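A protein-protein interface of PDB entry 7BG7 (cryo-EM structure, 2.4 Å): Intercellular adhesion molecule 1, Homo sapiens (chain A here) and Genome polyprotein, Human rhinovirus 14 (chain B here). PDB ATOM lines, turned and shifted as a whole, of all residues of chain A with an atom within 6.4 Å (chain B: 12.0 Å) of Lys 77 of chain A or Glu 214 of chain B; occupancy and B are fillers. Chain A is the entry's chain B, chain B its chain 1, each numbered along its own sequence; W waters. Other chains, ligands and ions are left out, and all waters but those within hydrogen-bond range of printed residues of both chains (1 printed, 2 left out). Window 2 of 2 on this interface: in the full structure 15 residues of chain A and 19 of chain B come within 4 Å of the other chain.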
ATOM      1  N   VAL A   4     -17.087 -30.495  24.394  1.00  0.00           N
ATOM      2  CA  VAL A   4     -16.001 -31.332  23.906  1.00  0.00           C
ATOM      3  C   VAL A   4     -16.449 -32.781  23.980  1.00  0.00           C
ATOM      4  O   VAL A   4     -17.072 -33.203  24.960  1.00  0.00           O
ATOM      5  CB  VAL A   4     -14.693 -31.122  24.697  1.00  0.00           C
ATOM      6  CG1 VAL A   4     -14.882 -31.471  26.166  1.00  0.00           C
ATOM      7  CG2 VAL A   4     -13.570 -31.947  24.092  1.00  0.00           C
ATOM      8  N   PRO A   6     -14.710 -36.784  23.230  1.00  0.00           N
ATOM      9  CA  PRO A   6     -15.402 -37.283  24.423  1.00  0.00           C
ATOM     10  C   PRO A   6     -15.162 -36.446  25.673  1.00  0.00           C
ATOM     11  O   PRO A   6     -14.153 -35.751  25.780  1.00  0.00           O
ATOM     12  CB  PRO A   6     -14.814 -38.688  24.603  1.00  0.00           C
ATOM     13  CG  PRO A   6     -14.155 -39.005  23.306  1.00  0.00           C
ATOM     14  CD  PRO A   6     -13.660 -37.713  22.795  1.00  0.00           C
ATOM     15  N   SER A   7     -16.106 -36.521  26.611  1.00  0.00           N
ATOM     16  CA  SER A   7     -15.896 -35.932  27.929  1.00  0.00           C
ATOM     17  C   SER A   7     -14.608 -36.450  28.544  1.00  0.00           C
ATOM     18  O   SER A   7     -13.878 -35.712  29.213  1.00  0.00           O
ATOM     19  CB  SER A   7     -17.088 -36.235  28.834  1.00  0.00           C
ATOM     20  OG  SER A   7     -18.085 -35.238  28.708  1.00  0.00           O
ATOM     21  N   GLU A  34      -7.218 -26.209  22.857  1.00  0.00           N
ATOM     22  CA  GLU A  34      -5.927 -25.832  23.414  1.00  0.00           C
ATOM     23  C   GLU A  34      -5.275 -27.063  24.020  1.00  0.00           C
ATOM     24  O   GLU A  34      -5.857 -27.713  24.894  1.00  0.00           O
ATOM     25  CB  GLU A  34      -6.071 -24.731  24.461  1.00  0.00           C
ATOM     26  CG  GLU A  34      -6.301 -23.361  23.864  1.00  0.00           C
ATOM     27  CD  GLU A  34      -5.747 -22.243  24.718  1.00  0.00           C
ATOM     28  OE1 GLU A  34      -5.506 -21.150  24.164  1.00  0.00           O
ATOM     29  OE2 GLU A  34      -5.558 -22.450  25.937  1.00  0.00           O
ATOM     30  N   GLN A  62      -5.188 -32.459  29.650  1.00  0.00           N
ATOM     31  CA  GLN A  62      -6.543 -31.918  29.761  1.00  0.00           C
ATOM     32  C   GLN A  62      -6.809 -30.928  28.630  1.00  0.00           C
ATOM     33  O   GLN A  62      -6.894 -29.715  28.852  1.00  0.00           O
ATOM     34  CB  GLN A  62      -6.742 -31.259  31.126  1.00  0.00           C
ATOM     35  CG  GLN A  62      -6.678 -32.236  32.297  1.00  0.00           C
ATOM     36  CD  GLN A  62      -5.253 -32.602  32.679  1.00  0.00           C
ATOM     37  OE1 GLN A  62      -4.368 -31.750  32.713  1.00  0.00           O
ATOM     38  NE2 GLN A  62      -5.026 -33.880  32.962  1.00  0.00           N
ATOM     39  N   PRO A  63      -6.958 -31.419  27.399  1.00  0.00           N
ATOM     40  CA  PRO A  63      -7.258 -30.524  26.273  1.00  0.00           C
ATOM     41  C   PRO A  63      -8.567 -29.780  26.493  1.00  0.00           C
ATOM     42  O   PRO A  63      -9.591 -30.373  26.834  1.00  0.00           O
ATOM     43  CB  PRO A  63      -7.351 -31.479  25.078  1.00  0.00           C
ATOM     44  CG  PRO A  63      -6.597 -32.680  25.487  1.00  0.00           C
ATOM     45  CD  PRO A  63      -6.831 -32.815  26.959  1.00  0.00           C
ATOM     46  N   MET A  64      -8.529 -28.473  26.276  1.00  0.00           N
ATOM     47  CA  MET A  64      -9.671 -27.601  26.499  1.00  0.00           C
ATOM     48  C   MET A  64     -10.174 -27.089  25.160  1.00  0.00           C
ATOM     49  O   MET A  64      -9.430 -26.435  24.425  1.00  0.00           O
ATOM     50  CB  MET A  64      -9.286 -26.436  27.409  1.00  0.00           C
ATOM     51  CG  MET A  64     -10.443 -25.539  27.792  1.00  0.00           C
ATOM     52  SD  MET A  64      -9.942 -24.153  28.826  1.00  0.00           S
ATOM     53  CE  MET A  64      -8.885 -23.254  27.694  1.00  0.00           C
ATOM     54  N   CYS A  65     -11.424 -27.405  24.831  1.00  0.00           N
ATOM     55  CA  CYS A  65     -12.070 -26.756  23.704  1.00  0.00           C
ATOM     56  C   CYS A  65     -12.446 -25.341  24.104  1.00  0.00           C
ATOM     57  O   CYS A  65     -12.931 -25.103  25.210  1.00  0.00           O
ATOM     58  CB  CYS A  65     -13.323 -27.520  23.274  1.00  0.00           C
ATOM     59  SG  CYS A  65     -13.023 -29.100  22.451  1.00  0.00           S
ATOM     60  N   TYR A  66     -12.197 -24.398  23.210  1.00  0.00           N
ATOM     61  CA  TYR A  66     -12.483 -22.998  23.471  1.00  0.00           C
ATOM     62  C   TYR A  66     -13.264 -22.389  22.317  1.00  0.00           C
ATOM     63  O   TYR A  66     -13.237 -22.887  21.190  1.00  0.00           O
ATOM     64  CB  TYR A  66     -11.194 -22.210  23.699  1.00  0.00           C
ATOM     65  CG  TYR A  66     -10.331 -22.105  22.470  1.00  0.00           C
ATOM     66  CD1 TYR A  66      -9.394 -23.082  22.175  1.00  0.00           C
ATOM     67  CD2 TYR A  66     -10.442 -21.026  21.611  1.00  0.00           C
ATOM     68  CE1 TYR A  66      -8.604 -22.995  21.057  1.00  0.00           C
ATOM     69  CE2 TYR A  66      -9.658 -20.931  20.490  1.00  0.00           C
ATOM     70  CZ  TYR A  66      -8.738 -21.917  20.218  1.00  0.00           C
ATOM     71  OH  TYR A  66      -7.951 -21.825  19.097  1.00  0.00           O
ATOM     72  N   GLN A  73     -20.846 -21.755  29.225  1.00  0.00           N
ATOM     73  CA  GLN A  73     -19.401 -21.836  29.371  1.00  0.00           C
ATOM     74  C   GLN A  73     -18.730 -21.885  28.004  1.00  0.00           C
ATOM     75  O   GLN A  73     -18.971 -22.792  27.205  1.00  0.00           O
ATOM     76  CB  GLN A  73     -19.025 -23.067  30.192  1.00  0.00           C
ATOM     77  CG  GLN A  73     -17.663 -22.979  30.866  1.00  0.00           C
ATOM     78  CD  GLN A  73     -17.646 -22.029  32.045  1.00  0.00           C
ATOM     79  OE1 GLN A  73     -18.602 -21.959  32.815  1.00  0.00           O
ATOM     80  NE2 GLN A  73     -16.557 -21.286  32.188  1.00  0.00           N
ATOM     81  N   SER A  74     -17.875 -20.899  27.743  1.00  0.00           N
ATOM     82  CA  SER A  74     -17.183 -20.775  26.469  1.00  0.00           C
ATOM     83  C   SER A  74     -15.992 -21.721  26.341  1.00  0.00           C
ATOM     84  O   SER A  74     -15.321 -21.707  25.305  1.00  0.00           O
ATOM     85  CB  SER A  74     -16.718 -19.330  26.266  1.00  0.00           C
ATOM     86  OG  SER A  74     -15.624 -19.024  27.110  1.00  0.00           O
ATOM     87  N   THR A  75     -15.710 -22.528  27.358  1.00  0.00           N
ATOM     88  CA  THR A  75     -14.608 -23.478  27.333  1.00  0.00           C
ATOM     89  C   THR A  75     -15.081 -24.795  27.926  1.00  0.00           C
ATOM     90  O   THR A  75     -15.933 -24.824  28.815  1.00  0.00           O
ATOM     91  CB  THR A  75     -13.374 -22.979  28.102  1.00  0.00           C
ATOM     92  OG1 THR A  75     -13.775 -22.440  29.365  1.00  0.00           O
ATOM     93  CG2 THR A  75     -12.623 -21.928  27.302  1.00  0.00           C
ATOM     94  N   ALA A  76     -14.516 -25.885  27.421  1.00  0.00           N
ATOM     95  CA  ALA A  76     -14.829 -27.223  27.900  1.00  0.00           C
ATOM     96  C   ALA A  76     -13.564 -28.062  27.888  1.00  0.00           C
ATOM     97  O   ALA A  76     -12.878 -28.142  26.867  1.00  0.00           O
ATOM     98  CB  ALA A  76     -15.909 -27.877  27.038  1.00  0.00           C
ATOM     99  N   LYS A  77     -13.262 -28.685  29.018  1.00  0.00           N
ATOM    100  CA  LYS A  77     -12.069 -29.505  29.157  1.00  0.00           C
ATOM    101  C   LYS A  77     -12.432 -30.977  29.067  1.00  0.00           C
ATOM    102  O   LYS A  77     -13.434 -31.419  29.633  1.00  0.00           O
ATOM    103  CB  LYS A  77     -11.369 -29.227  30.489  1.00  0.00           C
ATOM    104  CG  LYS A  77     -10.636 -27.906  30.546  1.00  0.00           C
ATOM    105  CD  LYS A  77      -9.584 -27.883  31.649  1.00  0.00           C
ATOM    106  CE  LYS A  77     -10.201 -27.972  33.033  1.00  0.00           C
ATOM    107  NZ  LYS A  77     -11.011 -26.764  33.371  1.00  0.00           N
ATOM    108  N   THR A  78     -11.626 -31.725  28.325  1.00  0.00           N
ATOM    109  CA  THR A  78     -11.678 -33.178  28.314  1.00  0.00           C
ATOM    110  C   THR A  78     -10.429 -33.725  28.991  1.00  0.00           C
ATOM    111  O   THR A  78      -9.399 -33.054  29.072  1.00  0.00           O
ATOM    112  CB  THR A  78     -11.791 -33.719  26.884  1.00  0.00           C
ATOM    113  OG1 THR A  78     -12.041 -35.130  26.924  1.00  0.00           O
ATOM    114  CG2 THR A  78     -10.519 -33.458  26.098  1.00  0.00           C
ATOM    115  N   PHE A  79     -10.529 -34.960  29.480  1.00  0.00           N
ATOM    116  CA  PHE A  79      -9.480 -35.570  30.289  1.00  0.00           C
ATOM    117  C   PHE A  79      -8.946 -36.809  29.580  1.00  0.00           C
ATOM    118  O   PHE A  79      -9.649 -37.817  29.464  1.00  0.00           O
ATOM    119  CB  PHE A  79     -10.015 -35.914  31.678  1.00  0.00           C
ATOM    120  CG  PHE A  79     -10.704 -34.764  32.354  1.00  0.00           C
ATOM    121  CD1 PHE A  79      -9.978 -33.809  33.039  1.00  0.00           C
ATOM    122  CD2 PHE A  79     -12.076 -34.632  32.291  1.00  0.00           C
ATOM    123  CE1 PHE A  79     -10.610 -32.747  33.656  1.00  0.00           C
ATOM    124  CE2 PHE A  79     -12.714 -33.570  32.904  1.00  0.00           C
ATOM    125  CZ  PHE A  79     -11.980 -32.627  33.586  1.00  0.00           C
ATOM    126  N   GLY B 207      -4.432 -10.183  27.125  1.00  0.00           N
ATOM    127  CA  GLY B 207      -5.716 -10.179  27.790  1.00  0.00           C
ATOM    128  C   GLY B 207      -6.601 -11.307  27.320  1.00  0.00           C
ATOM    129  O   GLY B 207      -6.179 -12.188  26.571  1.00  0.00           O
ATOM    130  N   TYR B 208      -7.849 -11.254  27.772  1.00  0.00           N
ATOM    131  CA  TYR B 208      -8.848 -12.270  27.500  1.00  0.00           C
ATOM    132  C   TYR B 208     -10.099 -11.604  26.956  1.00  0.00           C
ATOM    133  O   TYR B 208     -10.265 -10.388  27.036  1.00  0.00           O
ATOM    134  CB  TYR B 208      -9.193 -13.054  28.774  1.00  0.00           C
ATOM    135  CG  TYR B 208      -7.980 -13.602  29.460  1.00  0.00           C
ATOM    136  CD1 TYR B 208      -7.196 -12.794  30.259  1.00  0.00           C
ATOM    137  CD2 TYR B 208      -7.600 -14.922  29.291  1.00  0.00           C
ATOM    138  CE1 TYR B 208      -6.080 -13.277  30.869  1.00  0.00           C
ATOM    139  CE2 TYR B 208      -6.482 -15.421  29.908  1.00  0.00           C
ATOM    140  CZ  TYR B 208      -5.725 -14.593  30.697  1.00  0.00           C
ATOM    141  OH  TYR B 208      -4.603 -15.065  31.316  1.00  0.00           O
ATOM    142  N   SER B 209     -10.990 -12.419  26.395  1.00  0.00           N
ATOM    143  CA  SER B 209     -12.234 -11.884  25.861  1.00  0.00           C
ATOM    144  C   SER B 209     -13.144 -11.408  26.982  1.00  0.00           C
ATOM    145  O   SER B 209     -14.007 -10.556  26.757  1.00  0.00           O
ATOM    146  CB  SER B 209     -12.942 -12.923  24.996  1.00  0.00           C
ATOM    147  OG  SER B 209     -13.166 -14.118  25.708  1.00  0.00           O
ATOM    148  N   HIS B 210     -12.977 -11.963  28.179  1.00  0.00           N
ATOM    149  CA  HIS B 210     -13.754 -11.576  29.348  1.00  0.00           C
ATOM    150  C   HIS B 210     -13.109 -12.202  30.576  1.00  0.00           C
ATOM    151  O   HIS B 210     -12.274 -13.103  30.473  1.00  0.00           O
ATOM    152  CB  HIS B 210     -15.217 -12.003  29.204  1.00  0.00           C
ATOM    153  CG  HIS B 210     -15.415 -13.484  29.195  1.00  0.00           C
ATOM    154  ND1 HIS B 210     -14.758 -14.313  28.313  1.00  0.00           N
ATOM    155  CD2 HIS B 210     -16.205 -14.285  29.947  1.00  0.00           C
ATOM    156  CE1 HIS B 210     -15.129 -15.562  28.528  1.00  0.00           C
ATOM    157  NE2 HIS B 210     -16.009 -15.572  29.510  1.00  0.00           N
ATOM    158  N   ASP B 211     -13.525 -11.727  31.744  1.00  0.00           N
ATOM    159  CA  ASP B 211     -12.949 -12.146  33.022  1.00  0.00           C
ATOM    160  C   ASP B 211     -13.487 -13.519  33.402  1.00  0.00           C
ATOM    161  O   ASP B 211     -14.538 -13.657  34.025  1.00  0.00           O
ATOM    162  CB  ASP B 211     -13.247 -11.116  34.103  1.00  0.00           C
ATOM    163  CG  ASP B 211     -12.799  -9.722  33.715  1.00  0.00           C
ATOM    164  OD1 ASP B 211     -13.666  -8.881  33.411  1.00  0.00           O
ATOM    165  OD2 ASP B 211     -11.579  -9.470  33.699  1.00  0.00           O
ATOM    166  N   ASP B 212     -12.745 -14.549  33.006  1.00  0.00           N
ATOM    167  CA  ASP B 212     -13.115 -15.937  33.227  1.00  0.00           C
ATOM    168  C   ASP B 212     -11.843 -16.706  33.551  1.00  0.00           C
ATOM    169  O   ASP B 212     -10.758 -16.352  33.086  1.00  0.00           O
ATOM    170  CB  ASP B 212     -13.812 -16.518  31.992  1.00  0.00           C
ATOM    171  CG  ASP B 212     -14.197 -17.966  32.163  1.00  0.00           C
ATOM    172  OD1 ASP B 212     -14.817 -18.306  33.189  1.00  0.00           O
ATOM    173  OD2 ASP B 212     -13.883 -18.770  31.263  1.00  0.00           O
ATOM    174  N   ALA B 213     -11.983 -17.775  34.335  1.00  0.00           N
ATOM    175  CA  ALA B 213     -10.801 -18.496  34.796  1.00  0.00           C
ATOM    176  C   ALA B 213     -10.197 -19.385  33.719  1.00  0.00           C
ATOM    177  O   ALA B 213      -8.994 -19.666  33.760  1.00  0.00           O
ATOM    178  CB  ALA B 213     -11.151 -19.326  36.028  1.00  0.00           C
ATOM    179  N   GLU B 214     -10.995 -19.833  32.756  1.00  0.00           N
ATOM    180  CA  GLU B 214     -10.593 -20.886  31.839  1.00  0.00           C
ATOM    181  C   GLU B 214     -10.463 -20.392  30.408  1.00  0.00           C
ATOM    182  O   GLU B 214     -10.063 -21.164  29.534  1.00  0.00           O
ATOM    183  CB  GLU B 214     -11.585 -22.051  31.880  1.00  0.00           C
ATOM    184  CG  GLU B 214     -11.610 -22.821  33.182  1.00  0.00           C
ATOM    185  CD  GLU B 214     -12.660 -23.914  33.181  1.00  0.00           C
ATOM    186  OE1 GLU B 214     -13.487 -23.941  32.246  1.00  0.00           O
ATOM    187  OE2 GLU B 214     -12.650 -24.756  34.103  1.00  0.00           O
ATOM    188  N   THR B 215     -10.780 -19.129  30.150  1.00  0.00           N
ATOM    189  CA  THR B 215     -10.851 -18.636  28.788  1.00  0.00           C
ATOM    190  C   THR B 215      -9.461 -18.500  28.164  1.00  0.00           C
ATOM    191  O   THR B 215      -8.445 -18.341  28.844  1.00  0.00           O
ATOM    192  CB  THR B 215     -11.612 -17.308  28.743  1.00  0.00           C
ATOM    193  OG1 THR B 215     -11.719 -16.862  27.386  1.00  0.00           O
ATOM    194  CG2 THR B 215     -10.939 -16.244  29.593  1.00  0.00           C
ATOM    195  N   GLN B 216      -9.444 -18.562  26.836  1.00  0.00           N
ATOM    196  CA  GLN B 216      -8.209 -18.512  26.069  1.00  0.00           C
ATOM    197  C   GLN B 216      -7.488 -17.182  26.273  1.00  0.00           C
ATOM    198  O   GLN B 216      -8.108 -16.136  26.470  1.00  0.00           O
ATOM    199  CB  GLN B 216      -8.519 -18.729  24.582  1.00  0.00           C
ATOM    200  CG  GLN B 216      -9.477 -17.691  23.953  1.00  0.00           C
ATOM    201  CD  GLN B 216     -10.950 -17.982  24.210  1.00  0.00           C
ATOM    202  OE1 GLN B 216     -11.295 -18.946  24.891  1.00  0.00           O
ATOM    203  NE2 GLN B 216     -11.825 -17.145  23.669  1.00  0.00           N
ATOM    204  N   TYR B 217      -6.160 -17.236  26.209  1.00  0.00           N
ATOM    205  CA  TYR B 217      -5.294 -16.080  26.398  1.00  0.00           C
ATOM    206  C   TYR B 217      -4.698 -15.668  25.062  1.00  0.00           C
ATOM    207  O   TYR B 217      -4.332 -16.518  24.248  1.00  0.00           O
ATOM    208  CB  TYR B 217      -4.167 -16.401  27.383  1.00  0.00           C
ATOM    209  CG  TYR B 217      -3.143 -15.306  27.609  1.00  0.00           C
ATOM    210  CD1 TYR B 217      -3.499 -14.106  28.203  1.00  0.00           C
ATOM    211  CD2 TYR B 217      -1.818 -15.488  27.252  1.00  0.00           C
ATOM    212  CE1 TYR B 217      -2.563 -13.114  28.426  1.00  0.00           C
ATOM    213  CE2 TYR B 217      -0.874 -14.503  27.471  1.00  0.00           C
ATOM    214  CZ  TYR B 217      -1.249 -13.324  28.064  1.00  0.00           C
ATOM    215  OH  TYR B 217      -0.308 -12.348  28.280  1.00  0.00           O
ATOM    216  N   GLY B 218      -4.618 -14.363  24.832  1.00  0.00           N
ATOM    217  CA  GLY B 218      -3.910 -13.839  23.683  1.00  0.00           C
ATOM    218  C   GLY B 218      -4.749 -13.808  22.425  1.00  0.00           C
ATOM    219  O   GLY B 218      -5.088 -12.735  21.925  1.00  0.00           O
ATOM    220  N   ILE B 219      -5.072 -14.983  21.892  1.00  0.00           N
ATOM    221  CA  ILE B 219      -5.855 -15.056  20.668  1.00  0.00           C
ATOM    222  C   ILE B 219      -7.173 -14.324  20.884  1.00  0.00           C
ATOM    223  O   ILE B 219      -7.897 -14.593  21.849  1.00  0.00           O
ATOM    224  CB  ILE B 219      -6.060 -16.523  20.266  1.00  0.00           C
ATOM    225  CG1 ILE B 219      -6.618 -16.619  18.849  1.00  0.00           C
ATOM    226  CG2 ILE B 219      -6.963 -17.224  21.262  1.00  0.00           C
ATOM    227  CD1 ILE B 219      -6.503 -17.987  18.241  1.00  0.00           C
ATOM    228  N   ARG B 272      -0.355 -16.942  19.426  1.00  0.00           N
ATOM    229  CA  ARG B 272       0.331 -17.179  20.683  1.00  0.00           C
ATOM    230  C   ARG B 272       1.814 -16.906  20.521  1.00  0.00           C
ATOM    231  O   ARG B 272       2.380 -17.070  19.438  1.00  0.00           O
ATOM    232  CB  ARG B 272       0.120 -18.625  21.140  1.00  0.00           C
ATOM    233  CG  ARG B 272      -1.217 -18.880  21.788  1.00  0.00           C
ATOM    234  CD  ARG B 272      -2.251 -19.254  20.750  1.00  0.00           C
ATOM    235  NE  ARG B 272      -3.553 -19.521  21.348  1.00  0.00           N
ATOM    236  CZ  ARG B 272      -4.465 -20.339  20.837  1.00  0.00           C
ATOM    237  NH1 ARG B 272      -5.625 -20.493  21.453  1.00  0.00           N
ATOM    238  NH2 ARG B 272      -4.261 -20.934  19.671  1.00  0.00           N
HETATM  239  O   HOH W   1      -3.313 -19.006  24.365  1.00  0.00           O
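The side-chain amide oxygen (OE1) of Gln 216 of chain B is in hydrogen-bond range of the side-chain hydroxyl (OG1) of Thr 215 of chain B (3.3 Å). The side-chain carboxylate (OD2) of Asp 212 of chain B sits at hydrogen-bond distance from the backbone NH (N) of Thr 215 of chain B (3.3 Å). The side-chain carboxylate of Asp 212 of chain B sits close to the backbone NH of Glu 214 of chain B. O of Met 64 of chain A sits at hydrogen-bond distance from N of Glu 34 of chain A (2.7 Å). The side-chain hydroxyl (OG) of Ser 209 of chain B lies within hydrogen-bond range of a ring nitrogen (ND1) of His 210 of chain B, at 3.1 Å.
Of the 14 printed residues of chain B, 5 touch a printed residue of chain A. Printed residues of chain B that touch a printed residue of chain A: His 210, Asp 212, Glu 214, Gln 216 and Arg 272. Hydrophobic or aromatic side chains of chain B within 4 Å of the printed part of chain A: His 210. Of the 16 printed residues of chain A, 7 touch a printed residue of chain B.
Water W1 lies within hydrogen-bond range of O of Tyr 217 of chain B (2.7 Å), NE of Arg 272 of chain B (3.1 Å) and OE1 of Glu 34 of chain A (3.1 Å).
No residue of chain B comes within 4 Å of Ser 7 of chain A. Printed residues of chain B within 4 Å of Glu 34 of chain A: Gln 216 (3.9 Å) and Arg 272 (2.8 Å). No residue of chain B comes within 4 Å of Gln 62 of chain A. Met 64 of chain A touches just one residue of chain B: Glu 214 (3.0 Å). No residue of chain B comes within 4 Å of Cys 65 of chain A. Of the printed residues of chain B, Tyr 66 of chain A touches Gln 216 and Arg 272. Printed residues of chain B within 4 Å of Gln 73 of chain A: Asp 212 (3.6 Å). Ser 74 of chain A touches just one residue of chain B: His 210 (3.8 Å). Of chain B, only Glu 214 comes within 4 Å of Thr 75 of chain A. No residue of chain B comes within 4 Å of Ala 76 of chain A. Of chain B, only Glu 214 (2.7 Å) comes within 4 Å of Lys 77 of chain A. Printed residues of chain A within 4 Å of His 210 of chain B: Ser 74. Printed residues of chain A within 4 Å of Asp 212 of chain B: Gln 73. The nearest residue of chain B that does not touch Lys 77 of chain A is Ala 213 of chain B (7.4 Å). The nearest residue of chain A that does not touch Glu 214 of chain B is Gln 73 of chain A (4.1 Å).
Gln 216 of chain B touches Glu 34 of chain A. Gln 216 of chain B touches Tyr 66 of chain A (OE1 to CB, 3.5 Å). Arg 272 of chain B touches Tyr 66 of chain A (NH1 to OH, 3.6 Å). NE2 of Gln 73 of chain A touches OD1 of Asp 212 of chain B (3.6 Å). OG of Ser 74 of chain A touches CE1 of His 210 of chain B (3.8 Å).
The guanidinium group of Arg 272 of chain B is in salt-bridge range of the side-chain carboxylate of Glu 34 of chain A, at 2.8 Å. The side-chain sulfur (SD) of Met 64 of chain A lies close to the backbone carbonyl oxygen (O) of Glu 214 of chain B, 3.1 Å away. The side-chain amino group (NZ) of Lys 77 of chain A is in salt-bridge range of the side-chain carboxylate (OE2) of Glu 214 of chain B (2.7 Å). OE1 of Glu 214 of chain B sits at hydrogen-bond distance from OG1 of Thr 75 of chain A (3.3 Å).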
